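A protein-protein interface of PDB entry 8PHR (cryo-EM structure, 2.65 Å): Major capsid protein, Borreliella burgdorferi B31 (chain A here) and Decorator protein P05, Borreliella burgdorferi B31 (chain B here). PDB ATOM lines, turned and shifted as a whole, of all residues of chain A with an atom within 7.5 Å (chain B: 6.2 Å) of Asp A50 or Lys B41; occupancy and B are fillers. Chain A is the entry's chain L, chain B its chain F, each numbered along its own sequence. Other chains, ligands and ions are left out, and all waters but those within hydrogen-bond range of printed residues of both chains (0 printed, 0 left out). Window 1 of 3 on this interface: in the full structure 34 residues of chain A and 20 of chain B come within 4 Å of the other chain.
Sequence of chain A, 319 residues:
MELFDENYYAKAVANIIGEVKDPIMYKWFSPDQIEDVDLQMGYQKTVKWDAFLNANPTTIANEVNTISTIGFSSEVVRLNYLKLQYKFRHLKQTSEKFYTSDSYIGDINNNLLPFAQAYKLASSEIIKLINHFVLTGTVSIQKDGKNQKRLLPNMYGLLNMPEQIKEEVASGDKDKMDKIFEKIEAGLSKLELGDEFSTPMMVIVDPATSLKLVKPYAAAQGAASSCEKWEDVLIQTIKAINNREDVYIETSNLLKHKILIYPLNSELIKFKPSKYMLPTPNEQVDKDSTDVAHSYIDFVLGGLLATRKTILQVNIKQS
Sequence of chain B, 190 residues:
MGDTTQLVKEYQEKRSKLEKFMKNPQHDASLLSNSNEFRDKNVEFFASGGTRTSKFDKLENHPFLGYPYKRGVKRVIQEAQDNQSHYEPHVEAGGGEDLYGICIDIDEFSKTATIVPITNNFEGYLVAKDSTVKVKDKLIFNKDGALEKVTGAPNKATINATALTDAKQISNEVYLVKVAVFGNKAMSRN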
ATOM      1  N   LYS A  48      18.909 -16.301 -21.606  1.00  0.00           N
ATOM      2  CA  LYS A  48      18.003 -17.421 -21.813  1.00  0.00           C
ATOM      3  C   LYS A  48      18.711 -18.703 -21.403  1.00  0.00           C
ATOM      4  O   LYS A  48      19.830 -18.970 -21.859  1.00  0.00           O
ATOM      5  CB  LYS A  48      17.547 -17.503 -23.272  1.00  0.00           C
ATOM      6  CG  LYS A  48      16.762 -18.759 -23.611  1.00  0.00           C
ATOM      7  CD  LYS A  48      16.517 -18.864 -25.108  1.00  0.00           C
ATOM      8  CE  LYS A  48      15.757 -20.135 -25.457  1.00  0.00           C
ATOM      9  NZ  LYS A  48      15.465 -20.224 -26.914  1.00  0.00           N
ATOM     10  N   TRP A  49      18.063 -19.487 -20.547  1.00  0.00           N
ATOM     11  CA  TRP A  49      18.634 -20.704 -19.987  1.00  0.00           C
ATOM     12  C   TRP A  49      17.938 -21.916 -20.592  1.00  0.00           C
ATOM     13  O   TRP A  49      16.704 -21.981 -20.613  1.00  0.00           O
ATOM     14  CB  TRP A  49      18.490 -20.717 -18.464  1.00  0.00           C
ATOM     15  CG  TRP A  49      19.506 -19.875 -17.748  1.00  0.00           C
ATOM     16  CD1 TRP A  49      19.280 -18.693 -17.103  1.00  0.00           C
ATOM     17  CD2 TRP A  49      20.903 -20.154 -17.595  1.00  0.00           C
ATOM     18  NE1 TRP A  49      20.450 -18.217 -16.564  1.00  0.00           N
ATOM     19  CE2 TRP A  49      21.462 -19.095 -16.850  1.00  0.00           C
ATOM     20  CE3 TRP A  49      21.737 -21.194 -18.016  1.00  0.00           C
ATOM     21  CZ2 TRP A  49      22.814 -19.047 -16.518  1.00  0.00           C
ATOM     22  CZ3 TRP A  49      23.080 -21.145 -17.684  1.00  0.00           C
ATOM     23  CH2 TRP A  49      23.604 -20.079 -16.944  1.00  0.00           C
ATOM     24  N   ASP A  50      18.729 -22.876 -21.071  1.00  0.00           N
ATOM     25  CA  ASP A  50      18.215 -24.093 -21.682  1.00  0.00           C
ATOM     26  C   ASP A  50      18.857 -25.304 -21.020  1.00  0.00           C
ATOM     27  O   ASP A  50      19.938 -25.217 -20.432  1.00  0.00           O
ATOM     28  CB  ASP A  50      18.479 -24.124 -23.195  1.00  0.00           C
ATOM     29  CG  ASP A  50      17.568 -23.192 -23.969  1.00  0.00           C
ATOM     30  OD1 ASP A  50      16.696 -22.552 -23.345  1.00  0.00           O
ATOM     31  OD2 ASP A  50      17.724 -23.098 -25.204  1.00  0.00           O
ATOM     32  N   ALA A  51      18.178 -26.445 -21.127  1.00  0.00           N
ATOM     33  CA  ALA A  51      18.646 -27.692 -20.543  1.00  0.00           C
ATOM     34  C   ALA A  51      18.662 -28.786 -21.601  1.00  0.00           C
ATOM     35  O   ALA A  51      17.948 -28.720 -22.606  1.00  0.00           O
ATOM     36  CB  ALA A  51      17.774 -28.127 -19.358  1.00  0.00           C
ATOM     37  N   PHE A  52      19.491 -29.800 -21.361  1.00  0.00           N
ATOM     38  CA  PHE A  52      19.625 -30.915 -22.286  1.00  0.00           C
ATOM     39  C   PHE A  52      20.018 -32.169 -21.519  1.00  0.00           C
ATOM     40  O   PHE A  52      20.534 -32.101 -20.402  1.00  0.00           O
ATOM     41  CB  PHE A  52      20.649 -30.609 -23.389  1.00  0.00           C
ATOM     42  CG  PHE A  52      22.005 -30.212 -22.872  1.00  0.00           C
ATOM     43  CD1 PHE A  52      22.950 -31.173 -22.544  1.00  0.00           C
ATOM     44  CD2 PHE A  52      22.337 -28.876 -22.718  1.00  0.00           C
ATOM     45  CE1 PHE A  52      24.196 -30.807 -22.071  1.00  0.00           C
ATOM     46  CE2 PHE A  52      23.582 -28.505 -22.245  1.00  0.00           C
ATOM     47  CZ  PHE A  52      24.512 -29.472 -21.922  1.00  0.00           C
ATOM     48  N   LEU A  53      19.767 -33.319 -22.139  1.00  0.00           N
ATOM     49  CA  LEU A  53      20.104 -34.617 -21.572  1.00  0.00           C
ATOM     50  C   LEU A  53      21.420 -35.099 -22.167  1.00  0.00           C
ATOM     51  O   LEU A  53      21.670 -34.917 -23.363  1.00  0.00           O
ATOM     52  CB  LEU A  53      19.000 -35.638 -21.860  1.00  0.00           C
ATOM     53  CG  LEU A  53      17.559 -35.215 -21.567  1.00  0.00           C
ATOM     54  CD1 LEU A  53      16.595 -36.356 -21.857  1.00  0.00           C
ATOM     55  CD2 LEU A  53      17.407 -34.735 -20.136  1.00  0.00           C
ATOM     56  N   ASN A  54      22.265 -35.720 -21.338  1.00  0.00           N
ATOM     57  CA  ASN A  54      23.566 -36.165 -21.817  1.00  0.00           C
ATOM     58  C   ASN A  54      23.566 -37.598 -22.332  1.00  0.00           C
ATOM     59  O   ASN A  54      24.414 -37.937 -23.166  1.00  0.00           O
ATOM     60  CB  ASN A  54      24.612 -36.028 -20.709  1.00  0.00           C
ATOM     61  CG  ASN A  54      25.181 -34.625 -20.617  1.00  0.00           C
ATOM     62  OD1 ASN A  54      24.985 -33.927 -19.622  1.00  0.00           O
ATOM     63  ND2 ASN A  54      25.891 -34.206 -21.658  1.00  0.00           N
ATOM     64  N   ILE A  70      22.110 -34.224 -16.682  1.00  0.00           N
ATOM     65  CA  ILE A  70      21.394 -33.175 -17.394  1.00  0.00           C
ATOM     66  C   ILE A  70      22.250 -31.917 -17.349  1.00  0.00           C
ATOM     67  O   ILE A  70      22.580 -31.423 -16.263  1.00  0.00           O
ATOM     68  CB  ILE A  70      20.007 -32.916 -16.785  1.00  0.00           C
ATOM     69  CG1 ILE A  70      19.086 -34.110 -17.033  1.00  0.00           C
ATOM     70  CG2 ILE A  70      19.402 -31.641 -17.353  1.00  0.00           C
ATOM     71  CD1 ILE A  70      17.694 -33.934 -16.471  1.00  0.00           C
ATOM     72  N   GLY A  71      22.609 -31.402 -18.523  1.00  0.00           N
ATOM     73  CA  GLY A  71      23.412 -30.204 -18.624  1.00  0.00           C
ATOM     74  C   GLY A  71      22.574 -28.968 -18.921  1.00  0.00           C
ATOM     75  O   GLY A  71      21.417 -29.045 -19.324  1.00  0.00           O
ATOM     76  N   PHE A  72      23.200 -27.809 -18.724  1.00  0.00           N
ATOM     77  CA  PHE A  72      22.543 -26.526 -18.911  1.00  0.00           C
ATOM     78  C   PHE A  72      23.418 -25.617 -19.764  1.00  0.00           C
ATOM     79  O   PHE A  72      24.639 -25.778 -19.836  1.00  0.00           O
ATOM     80  CB  PHE A  72      22.232 -25.848 -17.566  1.00  0.00           C
ATOM     81  CG  PHE A  72      21.299 -26.636 -16.690  1.00  0.00           C
ATOM     82  CD1 PHE A  72      21.774 -27.668 -15.896  1.00  0.00           C
ATOM     83  CD2 PHE A  72      19.944 -26.348 -16.663  1.00  0.00           C
ATOM     84  CE1 PHE A  72      20.917 -28.394 -15.090  1.00  0.00           C
ATOM     85  CE2 PHE A  72      19.082 -27.072 -15.860  1.00  0.00           C
ATOM     86  CZ  PHE A  72      19.570 -28.095 -15.073  1.00  0.00           C
ATOM     87  N   SER A  73      22.769 -24.652 -20.413  1.00  0.00           N
ATOM     88  CA  SER A  73      23.450 -23.716 -21.296  1.00  0.00           C
ATOM     89  C   SER A  73      22.738 -22.373 -21.242  1.00  0.00           C
ATOM     90  O   SER A  73      21.561 -22.286 -20.885  1.00  0.00           O
ATOM     91  CB  SER A  73      23.499 -24.234 -22.737  1.00  0.00           C
ATOM     92  OG  SER A  73      22.205 -24.572 -23.203  1.00  0.00           O
ATOM     93  N   SER A  74      23.465 -21.321 -21.619  1.00  0.00           N
ATOM     94  CA  SER A  74      22.957 -19.960 -21.558  1.00  0.00           C
ATOM     95  C   SER A  74      23.216 -19.237 -22.871  1.00  0.00           C
ATOM     96  O   SER A  74      24.177 -19.531 -23.586  1.00  0.00           O
ATOM     97  CB  SER A  74      23.599 -19.168 -20.411  1.00  0.00           C
ATOM     98  OG  SER A  74      25.007 -19.109 -20.556  1.00  0.00           O
ATOM     99  N   GLU A  75      22.342 -18.280 -23.174  1.00  0.00           N
ATOM    100  CA  GLU A  75      22.506 -17.404 -24.325  1.00  0.00           C
ATOM    101  C   GLU A  75      22.219 -15.973 -23.895  1.00  0.00           C
ATOM    102  O   GLU A  75      21.270 -15.724 -23.147  1.00  0.00           O
ATOM    103  CB  GLU A  75      21.580 -17.810 -25.478  1.00  0.00           C
ATOM    104  CG  GLU A  75      21.803 -17.025 -26.759  1.00  0.00           C
ATOM    105  CD  GLU A  75      20.753 -17.312 -27.812  1.00  0.00           C
ATOM    106  OE1 GLU A  75      19.819 -18.090 -27.525  1.00  0.00           O
ATOM    107  OE2 GLU A  75      20.862 -16.760 -28.927  1.00  0.00           O
ATOM    108  N   SER B  33      18.306 -17.910 -30.377  1.00  0.00           N
ATOM    109  CA  SER B  33      18.380 -19.115 -31.186  1.00  0.00           C
ATOM    110  C   SER B  33      17.256 -20.069 -30.801  1.00  0.00           C
ATOM    111  O   SER B  33      16.778 -20.066 -29.663  1.00  0.00           O
ATOM    112  CB  SER B  33      19.734 -19.811 -31.017  1.00  0.00           C
ATOM    113  OG  SER B  33      19.777 -20.556 -29.813  1.00  0.00           O
ATOM    114  N   SER B  35      16.073 -23.760 -30.129  1.00  0.00           N
ATOM    115  CA  SER B  35      16.515 -25.100 -29.756  1.00  0.00           C
ATOM    116  C   SER B  35      15.402 -25.830 -29.018  1.00  0.00           C
ATOM    117  O   SER B  35      15.640 -26.519 -28.020  1.00  0.00           O
ATOM    118  CB  SER B  35      17.785 -25.048 -28.906  1.00  0.00           C
ATOM    119  OG  SER B  35      17.595 -24.245 -27.755  1.00  0.00           O
ATOM    120  N   ASN B  36      14.166 -25.682 -29.500  1.00  0.00           N
ATOM    121  CA  ASN B  36      13.027 -26.297 -28.827  1.00  0.00           C
ATOM    122  C   ASN B  36      13.077 -27.818 -28.899  1.00  0.00           C
ATOM    123  O   ASN B  36      12.646 -28.493 -27.957  1.00  0.00           O
ATOM    124  CB  ASN B  36      11.722 -25.779 -29.428  1.00  0.00           C
ATOM    125  CG  ASN B  36      11.489 -24.310 -29.135  1.00  0.00           C
ATOM    126  OD1 ASN B  36      12.256 -23.682 -28.403  1.00  0.00           O
ATOM    127  ND2 ASN B  36      10.429 -23.752 -29.707  1.00  0.00           N
ATOM    128  N   GLU B  37      13.580 -28.372 -30.001  1.00  0.00           N
ATOM    129  CA  GLU B  37      13.739 -29.816 -30.103  1.00  0.00           C
ATOM    130  C   GLU B  37      14.701 -30.310 -29.030  1.00  0.00           C
ATOM    131  O   GLU B  37      15.782 -29.747 -28.841  1.00  0.00           O
ATOM    132  CB  GLU B  37      14.248 -30.197 -31.492  1.00  0.00           C
ATOM    133  CG  GLU B  37      14.391 -31.694 -31.714  1.00  0.00           C
ATOM    134  CD  GLU B  37      15.339 -32.027 -32.849  1.00  0.00           C
ATOM    135  OE1 GLU B  37      15.938 -31.091 -33.419  1.00  0.00           O
ATOM    136  OE2 GLU B  37      15.485 -33.225 -33.170  1.00  0.00           O
ATOM    137  N   PHE B  38      14.307 -31.372 -28.332  1.00  0.00           N
ATOM    138  CA  PHE B  38      15.035 -31.866 -27.172  1.00  0.00           C
ATOM    139  C   PHE B  38      16.104 -32.891 -27.528  1.00  0.00           C
ATOM    140  O   PHE B  38      16.655 -33.531 -26.626  1.00  0.00           O
ATOM    141  CB  PHE B  38      14.061 -32.472 -26.157  1.00  0.00           C
ATOM    142  CG  PHE B  38      13.518 -33.813 -26.566  1.00  0.00           C
ATOM    143  CD1 PHE B  38      12.607 -33.923 -27.603  1.00  0.00           C
ATOM    144  CD2 PHE B  38      13.924 -34.966 -25.913  1.00  0.00           C
ATOM    145  CE1 PHE B  38      12.109 -35.155 -27.979  1.00  0.00           C
ATOM    146  CE2 PHE B  38      13.430 -36.200 -26.287  1.00  0.00           C
ATOM    147  CZ  PHE B  38      12.522 -36.294 -27.321  1.00  0.00           C
ATOM    148  N   ARG B  39      16.412 -33.064 -28.810  1.00  0.00           N
ATOM    149  CA  ARG B  39      17.364 -34.068 -29.257  1.00  0.00           C
ATOM    150  C   ARG B  39      18.605 -33.402 -29.837  1.00  0.00           C
ATOM    151  O   ARG B  39      18.520 -32.333 -30.449  1.00  0.00           O
ATOM    152  CB  ARG B  39      16.733 -34.998 -30.297  1.00  0.00           C
ATOM    153  CG  ARG B  39      15.463 -35.686 -29.820  1.00  0.00           C
ATOM    154  CD  ARG B  39      15.201 -36.973 -30.594  1.00  0.00           C
ATOM    155  NE  ARG B  39      15.027 -36.746 -32.024  1.00  0.00           N
ATOM    156  CZ  ARG B  39      13.992 -36.120 -32.572  1.00  0.00           C
ATOM    157  NH1 ARG B  39      12.993 -35.659 -31.837  1.00  0.00           N
ATOM    158  NH2 ARG B  39      13.957 -35.959 -33.891  1.00  0.00           N
ATOM    159  N   ASP B  40      19.756 -34.046 -29.631  1.00  0.00           N
ATOM    160  CA  ASP B  40      21.043 -33.585 -30.157  1.00  0.00           C
ATOM    161  C   ASP B  40      21.402 -32.192 -29.642  1.00  0.00           C
ATOM    162  O   ASP B  40      21.936 -31.357 -30.376  1.00  0.00           O
ATOM    163  CB  ASP B  40      21.060 -33.618 -31.687  1.00  0.00           C
ATOM    164  CG  ASP B  40      21.581 -34.932 -32.235  1.00  0.00           C
ATOM    165  OD1 ASP B  40      22.036 -35.773 -31.432  1.00  0.00           O
ATOM    166  OD2 ASP B  40      21.539 -35.122 -33.468  1.00  0.00           O
ATOM    167  N   LYS B  41      21.106 -31.935 -28.369  1.00  0.00           N
ATOM    168  CA  LYS B  41      21.522 -30.705 -27.707  1.00  0.00           C
ATOM    169  C   LYS B  41      22.726 -30.900 -26.796  1.00  0.00           C
ATOM    170  O   LYS B  41      23.178 -29.933 -26.176  1.00  0.00           O
ATOM    171  CB  LYS B  41      20.366 -30.118 -26.892  1.00  0.00           C
ATOM    172  CG  LYS B  41      19.106 -29.833 -27.682  1.00  0.00           C
ATOM    173  CD  LYS B  41      18.033 -29.245 -26.780  1.00  0.00           C
ATOM    174  CE  LYS B  41      18.513 -27.972 -26.100  1.00  0.00           C
ATOM    175  NZ  LYS B  41      17.469 -27.399 -25.206  1.00  0.00           N
ATOM    176  N   ASN B  42      23.256 -32.119 -26.697  1.00  0.00           N
ATOM    177  CA  ASN B  42      24.325 -32.415 -25.753  1.00  0.00           C
ATOM    178  C   ASN B  42      25.718 -32.341 -26.362  1.00  0.00           C
ATOM    179  O   ASN B  42      26.696 -32.235 -25.614  1.00  0.00           O
ATOM    180  CB  ASN B  42      24.122 -33.809 -25.144  1.00  0.00           C
ATOM    181  CG  ASN B  42      24.061 -34.901 -26.195  1.00  0.00           C
ATOM    182  OD1 ASN B  42      23.181 -34.901 -27.057  1.00  0.00           O
ATOM    183  ND2 ASN B  42      24.999 -35.840 -26.131  1.00  0.00           N
ATOM    184  N   VAL B  43      25.834 -32.391 -27.687  1.00  0.00           N
ATOM    185  CA  VAL B  43      27.141 -32.377 -28.348  1.00  0.00           C
ATOM    186  C   VAL B  43      27.547 -30.916 -28.542  1.00  0.00           C
ATOM    187  O   VAL B  43      27.333 -30.300 -29.588  1.00  0.00           O
ATOM    188  CB  VAL B  43      27.140 -33.200 -29.640  1.00  0.00           C
ATOM    189  CG1 VAL B  43      26.176 -32.649 -30.702  1.00  0.00           C
ATOM    190  CG2 VAL B  43      28.552 -33.293 -30.203  1.00  0.00           C
ATOM    191  N   GLU B  44      28.144 -30.348 -27.495  1.00  0.00           N
ATOM    192  CA  GLU B  44      28.634 -28.979 -27.513  1.00  0.00           C
ATOM    193  C   GLU B  44      29.939 -28.909 -26.735  1.00  0.00           C
ATOM    194  O   GLU B  44      30.206 -29.740 -25.863  1.00  0.00           O
ATOM    195  CB  GLU B  44      27.614 -27.997 -26.918  1.00  0.00           C
ATOM    196  CG  GLU B  44      26.306 -27.893 -27.692  1.00  0.00           C
ATOM    197  CD  GLU B  44      26.498 -27.324 -29.084  1.00  0.00           C
ATOM    198  OE1 GLU B  44      27.409 -26.490 -29.264  1.00  0.00           O
ATOM    199  OE2 GLU B  44      25.739 -27.714 -29.997  1.00  0.00           O
ATOM    200  N   PHE B  46      30.766 -26.675 -24.587  1.00  0.00           N
ATOM    201  CA  PHE B  46      30.535 -26.208 -23.228  1.00  0.00           C
ATOM    202  C   PHE B  46      29.897 -27.261 -22.331  1.00  0.00           C
ATOM    203  O   PHE B  46      29.650 -26.983 -21.154  1.00  0.00           O
ATOM    204  CB  PHE B  46      29.675 -24.934 -23.248  1.00  0.00           C
ATOM    205  CG  PHE B  46      28.356 -25.085 -23.967  1.00  0.00           C
ATOM    206  CD1 PHE B  46      27.336 -25.861 -23.440  1.00  0.00           C
ATOM    207  CD2 PHE B  46      28.140 -24.434 -25.169  1.00  0.00           C
ATOM    208  CE1 PHE B  46      26.132 -25.994 -24.104  1.00  0.00           C
ATOM    209  CE2 PHE B  46      26.936 -24.560 -25.837  1.00  0.00           C
ATOM    210  CZ  PHE B  46      25.931 -25.340 -25.302  1.00  0.00           C
ATOM    211  N   ALA B  47      29.623 -28.454 -22.854  1.00  0.00           N
ATOM    212  CA  ALA B  47      29.029 -29.532 -22.066  1.00  0.00           C
ATOM    213  C   ALA B  47      30.111 -30.119 -21.169  1.00  0.00           C
ATOM    214  O   ALA B  47      30.813 -31.064 -21.533  1.00  0.00           O
ATOM    215  CB  ALA B  47      28.416 -30.592 -22.972  1.00  0.00           C
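O of Ala A51 is in hydrogen-bond range of NZ of Lys B41 (3.0 Å). The backbone carbonyl oxygen (O) of Ser B33 sits at hydrogen-bond distance from the side-chain amino group (NZ) of Lys A48, at 3.1 Å. N of Ser B33 lies within hydrogen-bond range of OE2 of Glu A75 (3.2 Å). The side-chain carboxylate (OD2) of Asp A50 sits at hydrogen-bond distance from the side-chain hydroxyl (OG) of Ser B35 (2.8 Å).
The backbone NH (N) of Lys A48 lies within hydrogen-bond range of the backbone carbonyl oxygen (O) of Glu A75, 2.9 Å away. The backbone NH of Ser A73 sits at hydrogen-bond distance from the backbone carbonyl oxygen of Asp A50. The side-chain amino group of Lys B41 sits at hydrogen-bond distance from the backbone carbonyl oxygen of Ser B35, 3.5 Å away. The backbone carbonyl oxygen of Phe A52 sits at hydrogen-bond distance from the backbone NH of Gly A71.
Among the printed residues, merely in contact across the chains: Leu A53 with Asn B42 (3.2 Å), Ser A73 with Phe B46 (3.4 Å), Phe A52 with Lys B41 (3.5 Å), Asn A54 with Asn B42 (3.7 Å), Phe A52 with Asn B42 (3.7 Å) and Asp A50 with Lys B41 (3.97 Å).
Printed residues of chain B within 4 Å of Asp A50: Ser B35 and Lys B41. Printed residues of chain B within 4 Å of Ala A51: Lys B41. Printed residues of chain B within 4 Å of Glu A75: Ser B33. Printed residues of chain A within 4 Å of Ser B35: Asp A50 (2.8 Å). Of the printed residues of chain A, Lys B41 touches Asp A50, Ala A51 and Phe A52. Printed residues of chain A within 4 Å of Phe B46: Ser A73 (3.4 Å).
Of the 13 printed residues of chain A, 8 touch a printed residue of chain B. Along chain B the printed residues that touch a printed residue of chain A span positions 33 to 46. Among the printed residues, 10 pairs touch across the chains. Among the printed residues, no Asp or Glu carboxylate lies within 4 Å of a Lys or Arg side-chain nitrogen of the other chain.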
